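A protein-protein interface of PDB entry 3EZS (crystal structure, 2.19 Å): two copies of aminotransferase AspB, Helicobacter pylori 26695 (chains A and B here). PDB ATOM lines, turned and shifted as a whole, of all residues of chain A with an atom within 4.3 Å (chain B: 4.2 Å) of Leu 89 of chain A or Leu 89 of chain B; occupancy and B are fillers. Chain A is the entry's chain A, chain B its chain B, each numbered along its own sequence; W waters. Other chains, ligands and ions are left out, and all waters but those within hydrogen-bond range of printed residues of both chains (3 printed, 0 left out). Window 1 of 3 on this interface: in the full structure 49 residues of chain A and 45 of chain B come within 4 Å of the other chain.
OG1 of Thr 263 of chain B sits at hydrogen-bond distance from NE of Arg 239 of chain A (2.9 Å).
The guanidinium group (NE) of Arg 239 of chain B sits at hydrogen-bond distance from the side-chain hydroxyl (OG1) of Thr 263 of chain A (2.9 Å).
Of the 11 printed residues of chain B, 6 touch a printed residue of chain A.
Hydrophobic or aromatic side chains of chain B that line the printed part of chain A: Leu 89 and Tyr 262.
Among the printed residues, 9 pairs touch across the chains.
Among the printed residues, no Asp or Glu carboxylate lies within 4 Å of a Lys or Arg side-chain nitrogen of the other chain.
Water W3 lies within hydrogen-bond range of the backbone carbonyl oxygen (O) of Leu 89 of chain B (2.6 Å), the backbone carbonyl oxygen (O) of Gly 261 of chain A (2.7 Å), the guanidinium group (NH2) of Arg 239 of chain B (3.1 Å) and the backbone NH (N) of Glu 93 of chain B (3.4 Å).
Water W1 lies within hydrogen-bond range of the backbone carbonyl oxygen (O) of Leu 89 of chain A, the backbone carbonyl oxygen (O) of Gly 261 of chain B, the guanidinium group (NH2) of Arg 239 of chain A and the backbone NH (N) of Glu 93 of chain A.
Water W2 lies within hydrogen-bond range of OG1 of Thr 263 of chain A (2.9 Å) and NH2 of Arg 239 of chain B (3.0 Å).
The side-chain carboxylate of Glu 93 of chain B sits at hydrogen-bond distance from the backbone NH of Leu 89 of chain B (3.0 Å).
The guanidinium group (NH2) of Arg 257 of chain B is in salt-bridge range of the side-chain carboxylate (OE2) of Glu 93 of chain B, 2.8 Å away.
The backbone NH (N) of Gly 90 of chain A lies within hydrogen-bond range of the backbone carbonyl oxygen (O) of Arg 239 of chain A, at 3.3 Å.
The backbone NH (N) of Leu 89 of chain A sits at hydrogen-bond distance from the side-chain carboxylate (OE2) of Glu 93 of chain A.
O of Arg 239 of chain B sits at hydrogen-bond distance from N of Gly 90 of chain B (3.2 Å).
Leu 89 of chain B touches its own counterpart, Leu 89 of chain A.
Leu 89 of chain A touches Thr 263 of chain B, and with the chains exchanged Thr 263 of chain A touches Leu 89 of chain B.
Arg 239 of chain A touches Thr 263 of chain B, and with the chains exchanged Thr 263 of chain A touches Arg 239 of chain B.
Gly 261 of chain A touches Glu 93 of chain B, but with the chains exchanged Glu 93 of chain A does not touch Gly 261 of chain B (4.3 Å).
Of the 9 pairs that touch across the chains among the printed residues, 8 have their exchanged pair printed and touching as well.
Among the printed residues, pairs that only touch across the chains: Tyr 262 of chain A with Tyr 262 of chain B (3.2 Å), Leu 89 of chain A with Leu 89 of chain B (3.7 Å), Gly 261 of chain A with Tyr 262 of chain B (3.8 Å), Tyr 262 of chain A with Gly 261 of chain B (3.9 Å), Leu 89 of chain A with Thr 263 of chain B (3.9 Å), Thr 263 of chain A with Leu 89 of chain B (3.9 Å) and Gly 261 of chain A with Glu 93 of chain B (3.97 Å).
Phe 60 of chain A touches none of the printed residues of chain B.
Of the printed residues of chain B, Leu 89 of chain A touches Leu 89 and Thr 263.
Of the printed residues of chain B, Arg 239 of chain A touches Thr 263.
Thr 88 of chain B touches none of the printed residues of chain A.
Of chain A, only Leu 89 (3.7 Å) and Thr 263 (3.9 Å) come within 4 Å of Leu 89 of chain B.
Printed residues of chain A within 4 Å of Glu 93 of chain B: Gly 261 (3.97 Å).
Printed residues of chain A within 4 Å of Arg 239 of chain B: Thr 263.
Of the printed residues of chain A, Tyr 262 of chain B touches Gly 261 and Tyr 262.
The nearest residue of chain B that does not touch Leu 89 of chain A is Gly 261 of chain B (4.1 Å).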
ATOM      1  N   PHE A  60      19.573 -20.463  22.326  1.00  0.00           N
ATOM      2  CA  PHE A  60      18.558 -20.784  23.331  1.00  0.00           C
ATOM      3  C   PHE A  60      18.583 -22.298  23.578  1.00  0.00           C
ATOM      4  O   PHE A  60      19.169 -23.050  22.817  1.00  0.00           O
ATOM      5  CB  PHE A  60      17.151 -20.315  22.928  1.00  0.00           C
ATOM      6  CG  PHE A  60      17.002 -18.818  22.835  1.00  0.00           C
ATOM      7  CD1 PHE A  60      17.458 -18.130  21.737  1.00  0.00           C
ATOM      8  CD2 PHE A  60      16.367 -18.110  23.841  1.00  0.00           C
ATOM      9  CE1 PHE A  60      17.307 -16.766  21.637  1.00  0.00           C
ATOM     10  CE2 PHE A  60      16.218 -16.735  23.753  1.00  0.00           C
ATOM     11  CZ  PHE A  60      16.681 -16.064  22.644  1.00  0.00           C
ATOM     12  N   THR A  88      14.319 -16.822  18.982  1.00  0.00           N
ATOM     13  CA  THR A  88      14.726 -15.413  19.032  1.00  0.00           C
ATOM     14  C   THR A  88      14.170 -14.670  20.265  1.00  0.00           C
ATOM     15  O   THR A  88      13.299 -15.172  20.970  1.00  0.00           O
ATOM     16  CB  THR A  88      14.282 -14.685  17.738  1.00  0.00           C
ATOM     17  OG1 THR A  88      12.854 -14.561  17.712  1.00  0.00           O
ATOM     18  CG2 THR A  88      14.738 -15.448  16.505  1.00  0.00           C
ATOM     19  N   LEU A  89      14.689 -13.466  20.494  1.00  0.00           N
ATOM     20  CA  LEU A  89      14.326 -12.655  21.642  1.00  0.00           C
ATOM     21  C   LEU A  89      13.132 -11.772  21.278  1.00  0.00           C
ATOM     22  O   LEU A  89      13.226 -10.553  21.272  1.00  0.00           O
ATOM     23  CB  LEU A  89      15.539 -11.806  22.075  1.00  0.00           C
ATOM     24  CG  LEU A  89      15.536 -11.370  23.536  1.00  0.00           C
ATOM     25  CD1 LEU A  89      15.743 -12.635  24.397  1.00  0.00           C
ATOM     26  CD2 LEU A  89      16.593 -10.336  23.822  1.00  0.00           C
ATOM     27  N   GLY A  90      11.991 -12.401  21.013  1.00  0.00           N
ATOM     28  CA  GLY A  90      10.816 -11.690  20.521  1.00  0.00           C
ATOM     29  C   GLY A  90      10.940 -11.553  19.011  1.00  0.00           C
ATOM     30  O   GLY A  90      11.865 -12.097  18.410  1.00  0.00           O
ATOM     31  N   GLU A  93      13.492  -7.629  17.250  1.00  0.00           N
ATOM     32  CA  GLU A  93      14.894  -7.694  16.867  1.00  0.00           C
ATOM     33  C   GLU A  93      15.134  -8.461  15.569  1.00  0.00           C
ATOM     34  O   GLU A  93      15.957  -8.053  14.763  1.00  0.00           O
ATOM     35  CB  GLU A  93      15.699  -8.290  18.022  1.00  0.00           C
ATOM     36  CG  GLU A  93      15.309  -9.714  18.477  1.00  0.00           C
ATOM     37  CD  GLU A  93      16.223 -10.806  17.951  1.00  0.00           C
ATOM     38  OE1 GLU A  93      16.942 -10.597  16.963  1.00  0.00           O
ATOM     39  OE2 GLU A  93      16.228 -11.887  18.557  1.00  0.00           O
ATOM     40  N   ARG A 239      10.013 -12.013  26.165  1.00  0.00           N
ATOM     41  CA  ARG A 239      10.818 -11.731  24.978  1.00  0.00           C
ATOM     42  C   ARG A 239      11.133 -13.042  24.266  1.00  0.00           C
ATOM     43  O   ARG A 239      12.291 -13.418  24.120  1.00  0.00           O
ATOM     44  CB  ARG A 239      12.125 -10.987  25.322  1.00  0.00           C
ATOM     45  CG  ARG A 239      12.014  -9.802  26.259  1.00  0.00           C
ATOM     46  CD  ARG A 239      11.046  -8.691  25.816  1.00  0.00           C
ATOM     47  NE  ARG A 239      11.183  -8.320  24.410  1.00  0.00           N
ATOM     48  CZ  ARG A 239      10.269  -8.450  23.447  1.00  0.00           C
ATOM     49  NH1 ARG A 239       9.053  -8.934  23.663  1.00  0.00           N
ATOM     50  NH2 ARG A 239      10.593  -8.061  22.225  1.00  0.00           N
ATOM     51  N   ARG A 257      24.037 -14.709  14.500  1.00  0.00           N
ATOM     52  CA  ARG A 257      23.456 -14.468  15.817  1.00  0.00           C
ATOM     53  C   ARG A 257      24.386 -14.760  17.001  1.00  0.00           C
ATOM     54  O   ARG A 257      24.161 -14.255  18.108  1.00  0.00           O
ATOM     55  CB  ARG A 257      22.149 -15.248  15.962  1.00  0.00           C
ATOM     56  CG  ARG A 257      20.984 -14.671  15.149  1.00  0.00           C
ATOM     57  CD  ARG A 257      19.666 -15.434  15.415  1.00  0.00           C
ATOM     58  NE  ARG A 257      19.180 -15.194  16.766  1.00  0.00           N
ATOM     59  CZ  ARG A 257      18.435 -14.146  17.137  1.00  0.00           C
ATOM     60  NH1 ARG A 257      18.068 -13.221  16.272  1.00  0.00           N
ATOM     61  NH2 ARG A 257      18.072 -14.017  18.398  1.00  0.00           N
ATOM     62  N   GLY A 261      24.413 -11.115  20.885  1.00  0.00           N
ATOM     63  CA  GLY A 261      24.098 -11.000  22.309  1.00  0.00           C
ATOM     64  C   GLY A 261      22.622 -10.856  22.653  1.00  0.00           C
ATOM     65  O   GLY A 261      22.270 -10.211  23.663  1.00  0.00           O
ATOM     66  N   TYR A 262      21.758 -11.431  21.818  1.00  0.00           N
ATOM     67  CA  TYR A 262      20.316 -11.455  22.082  1.00  0.00           C
ATOM     68  C   TYR A 262      19.968 -12.715  22.893  1.00  0.00           C
ATOM     69  O   TYR A 262      19.309 -13.631  22.385  1.00  0.00           O
ATOM     70  CB  TYR A 262      19.499 -11.454  20.786  1.00  0.00           C
ATOM     71  CG  TYR A 262      19.414 -10.138  20.042  1.00  0.00           C
ATOM     72  CD1 TYR A 262      18.565  -9.129  20.483  1.00  0.00           C
ATOM     73  CD2 TYR A 262      20.130  -9.927  18.860  1.00  0.00           C
ATOM     74  CE1 TYR A 262      18.456  -7.937  19.799  1.00  0.00           C
ATOM     75  CE2 TYR A 262      20.015  -8.733  18.152  1.00  0.00           C
ATOM     76  CZ  TYR A 262      19.170  -7.738  18.631  1.00  0.00           C
ATOM     77  OH  TYR A 262      19.042  -6.541  17.941  1.00  0.00           O
ATOM     78  N   THR A 263      20.388 -12.746  24.157  1.00  0.00           N
ATOM     79  CA  THR A 263      20.176 -13.918  25.006  1.00  0.00           C
ATOM     80  C   THR A 263      19.285 -13.596  26.207  1.00  0.00           C
ATOM     81  O   THR A 263      19.059 -12.433  26.557  1.00  0.00           O
ATOM     82  CB  THR A 263      21.509 -14.501  25.464  1.00  0.00           C
ATOM     83  OG1 THR A 263      22.207 -13.504  26.192  1.00  0.00           O
ATOM     84  CG2 THR A 263      22.379 -14.930  24.247  1.00  0.00           C
ATOM     85  N   SER A 264      18.783 -14.660  26.825  1.00  0.00           N
ATOM     86  CA  SER A 264      17.822 -14.568  27.910  1.00  0.00           C
ATOM     87  C   SER A 264      18.127 -15.613  28.992  1.00  0.00           C
ATOM     88  O   SER A 264      18.620 -16.691  28.690  1.00  0.00           O
ATOM     89  CB  SER A 264      16.446 -14.828  27.297  1.00  0.00           C
ATOM     90  OG  SER A 264      15.411 -14.424  28.150  1.00  0.00           O
ATOM     91  N   PHE B  60      15.192   0.599  29.555  1.00  0.00           N
ATOM     92  CA  PHE B  60      15.101  -0.130  30.841  1.00  0.00           C
ATOM     93  C   PHE B  60      14.416   0.775  31.891  1.00  0.00           C
ATOM     94  O   PHE B  60      14.155   1.934  31.636  1.00  0.00           O
ATOM     95  CB  PHE B  60      16.446  -0.687  31.342  1.00  0.00           C
ATOM     96  CG  PHE B  60      17.046  -1.755  30.451  1.00  0.00           C
ATOM     97  CD1 PHE B  60      17.628  -1.426  29.234  1.00  0.00           C
ATOM     98  CD2 PHE B  60      17.059  -3.075  30.845  1.00  0.00           C
ATOM     99  CE1 PHE B  60      18.196  -2.400  28.428  1.00  0.00           C
ATOM    100  CE2 PHE B  60      17.625  -4.047  30.046  1.00  0.00           C
ATOM    101  CZ  PHE B  60      18.190  -3.708  28.830  1.00  0.00           C
ATOM    102  N   THR B  88      21.946  -1.616  29.411  1.00  0.00           N
ATOM    103  CA  THR B  88      22.089  -2.555  28.307  1.00  0.00           C
ATOM    104  C   THR B  88      21.845  -4.019  28.742  1.00  0.00           C
ATOM    105  O   THR B  88      21.803  -4.367  29.939  1.00  0.00           O
ATOM    106  CB  THR B  88      23.506  -2.431  27.632  1.00  0.00           C
ATOM    107  OG1 THR B  88      24.557  -2.779  28.561  1.00  0.00           O
ATOM    108  CG2 THR B  88      23.767  -0.979  27.060  1.00  0.00           C
ATOM    109  N   LEU B  89      21.707  -4.878  27.743  1.00  0.00           N
ATOM    110  CA  LEU B  89      21.463  -6.302  27.949  1.00  0.00           C
ATOM    111  C   LEU B  89      22.829  -6.999  28.076  1.00  0.00           C
ATOM    112  O   LEU B  89      23.197  -7.854  27.261  1.00  0.00           O
ATOM    113  CB  LEU B  89      20.636  -6.848  26.774  1.00  0.00           C
ATOM    114  CG  LEU B  89      19.754  -8.041  27.052  1.00  0.00           C
ATOM    115  CD1 LEU B  89      18.648  -7.620  28.032  1.00  0.00           C
ATOM    116  CD2 LEU B  89      19.159  -8.575  25.743  1.00  0.00           C
ATOM    117  N   GLY B  90      23.570  -6.624  29.121  1.00  0.00           N
ATOM    118  CA  GLY B  90      24.924  -7.117  29.336  1.00  0.00           C
ATOM    119  C   GLY B  90      25.873  -6.282  28.487  1.00  0.00           C
ATOM    120  O   GLY B  90      25.472  -5.248  27.934  1.00  0.00           O
ATOM    121  N   GLU B  93      26.410  -7.398  23.622  1.00  0.00           N
ATOM    122  CA  GLU B  93      25.682  -6.747  22.544  1.00  0.00           C
ATOM    123  C   GLU B  93      26.178  -5.326  22.289  1.00  0.00           C
ATOM    124  O   GLU B  93      26.289  -4.903  21.128  1.00  0.00           O
ATOM    125  CB  GLU B  93      24.163  -6.834  22.764  1.00  0.00           C
ATOM    126  CG  GLU B  93      23.586  -6.214  24.066  1.00  0.00           C
ATOM    127  CD  GLU B  93      23.144  -4.749  23.930  1.00  0.00           C
ATOM    128  OE1 GLU B  93      23.438  -4.078  22.898  1.00  0.00           O
ATOM    129  OE2 GLU B  93      22.472  -4.284  24.878  1.00  0.00           O
ATOM    130  N   ARG B 239      21.552 -10.794  32.365  1.00  0.00           N
ATOM    131  CA  ARG B 239      21.863 -10.002  31.157  1.00  0.00           C
ATOM    132  C   ARG B 239      21.819  -8.499  31.436  1.00  0.00           C
ATOM    133  O   ARG B 239      21.095  -7.777  30.760  1.00  0.00           O
ATOM    134  CB  ARG B 239      20.928 -10.315  29.976  1.00  0.00           C
ATOM    135  CG  ARG B 239      20.722 -11.768  29.628  1.00  0.00           C
ATOM    136  CD  ARG B 239      21.977 -12.551  29.318  1.00  0.00           C
ATOM    137  NE  ARG B 239      22.922 -11.877  28.435  1.00  0.00           N
ATOM    138  CZ  ARG B 239      24.188 -11.574  28.725  1.00  0.00           C
ATOM    139  NH1 ARG B 239      24.750 -11.894  29.887  1.00  0.00           N
ATOM    140  NH2 ARG B 239      24.922 -10.962  27.810  1.00  0.00           N
ATOM    141  N   ARG B 257      19.005   2.473  19.823  1.00  0.00           N
ATOM    142  CA  ARG B 257      18.605   1.310  20.606  1.00  0.00           C
ATOM    143  C   ARG B 257      17.089   1.043  20.625  1.00  0.00           C
ATOM    144  O   ARG B 257      16.657  -0.116  20.830  1.00  0.00           O
ATOM    145  CB  ARG B 257      19.159   1.411  22.033  1.00  0.00           C
ATOM    146  CG  ARG B 257      20.673   1.233  22.107  1.00  0.00           C
ATOM    147  CD  ARG B 257      21.188   1.217  23.530  1.00  0.00           C
ATOM    148  NE  ARG B 257      20.680   0.067  24.280  1.00  0.00           N
ATOM    149  CZ  ARG B 257      21.207  -1.157  24.265  1.00  0.00           C
ATOM    150  NH1 ARG B 257      22.259  -1.433  23.521  1.00  0.00           N
ATOM    151  NH2 ARG B 257      20.649  -2.125  24.992  1.00  0.00           N
ATOM    152  N   GLY B 261      15.712  -3.913  19.878  1.00  0.00           N
ATOM    153  CA  GLY B 261      14.989  -4.953  20.614  1.00  0.00           C
ATOM    154  C   GLY B 261      15.763  -5.698  21.702  1.00  0.00           C
ATOM    155  O   GLY B 261      15.421  -6.827  22.030  1.00  0.00           O
ATOM    156  N   TYR B 262      16.795  -5.079  22.259  1.00  0.00           N
ATOM    157  CA  TYR B 262      17.555  -5.683  23.354  1.00  0.00           C
ATOM    158  C   TYR B 262      16.882  -5.331  24.687  1.00  0.00           C
ATOM    159  O   TYR B 262      17.419  -4.521  25.456  1.00  0.00           O
ATOM    160  CB  TYR B 262      18.991  -5.167  23.393  1.00  0.00           C
ATOM    161  CG  TYR B 262      19.888  -5.651  22.292  1.00  0.00           C
ATOM    162  CD1 TYR B 262      20.415  -6.935  22.332  1.00  0.00           C
ATOM    163  CD2 TYR B 262      20.275  -4.813  21.262  1.00  0.00           C
ATOM    164  CE1 TYR B 262      21.275  -7.382  21.367  1.00  0.00           C
ATOM    165  CE2 TYR B 262      21.146  -5.255  20.272  1.00  0.00           C
ATOM    166  CZ  TYR B 262      21.644  -6.544  20.330  1.00  0.00           C
ATOM    167  OH  TYR B 262      22.506  -7.020  19.358  1.00  0.00           O
ATOM    168  N   THR B 263      15.725  -5.950  24.952  1.00  0.00           N
ATOM    169  CA  THR B 263      14.941  -5.662  26.145  1.00  0.00           C
ATOM    170  C   THR B 263      14.860  -6.877  27.064  1.00  0.00           C
ATOM    171  O   THR B 263      15.135  -8.014  26.647  1.00  0.00           O
ATOM    172  CB  THR B 263      13.559  -5.119  25.788  1.00  0.00           C
ATOM    173  OG1 THR B 263      12.881  -6.059  24.968  1.00  0.00           O
ATOM    174  CG2 THR B 263      13.665  -3.782  25.028  1.00  0.00           C
ATOM    175  N   SER B 264      14.454  -6.603  28.309  1.00  0.00           N
ATOM    176  CA  SER B 264      14.468  -7.567  29.412  1.00  0.00           C
ATOM    177  C   SER B 264      13.228  -7.447  30.314  1.00  0.00           C
ATOM    178  O   SER B 264      12.828  -6.325  30.658  1.00  0.00           O
ATOM    179  CB  SER B 264      15.705  -7.204  30.233  1.00  0.00           C
ATOM    180  OG  SER B 264      16.003  -8.151  31.196  1.00  0.00           O
HETATM  181  O   HOH W   1      13.271  -7.997  20.544  1.00  0.00           O
HETATM  182  O   HOH W   2      24.839 -12.678  25.362  1.00  0.00           O
HETATM  183  O   HOH W   3      24.154  -9.249  25.350  1.00  0.00           O
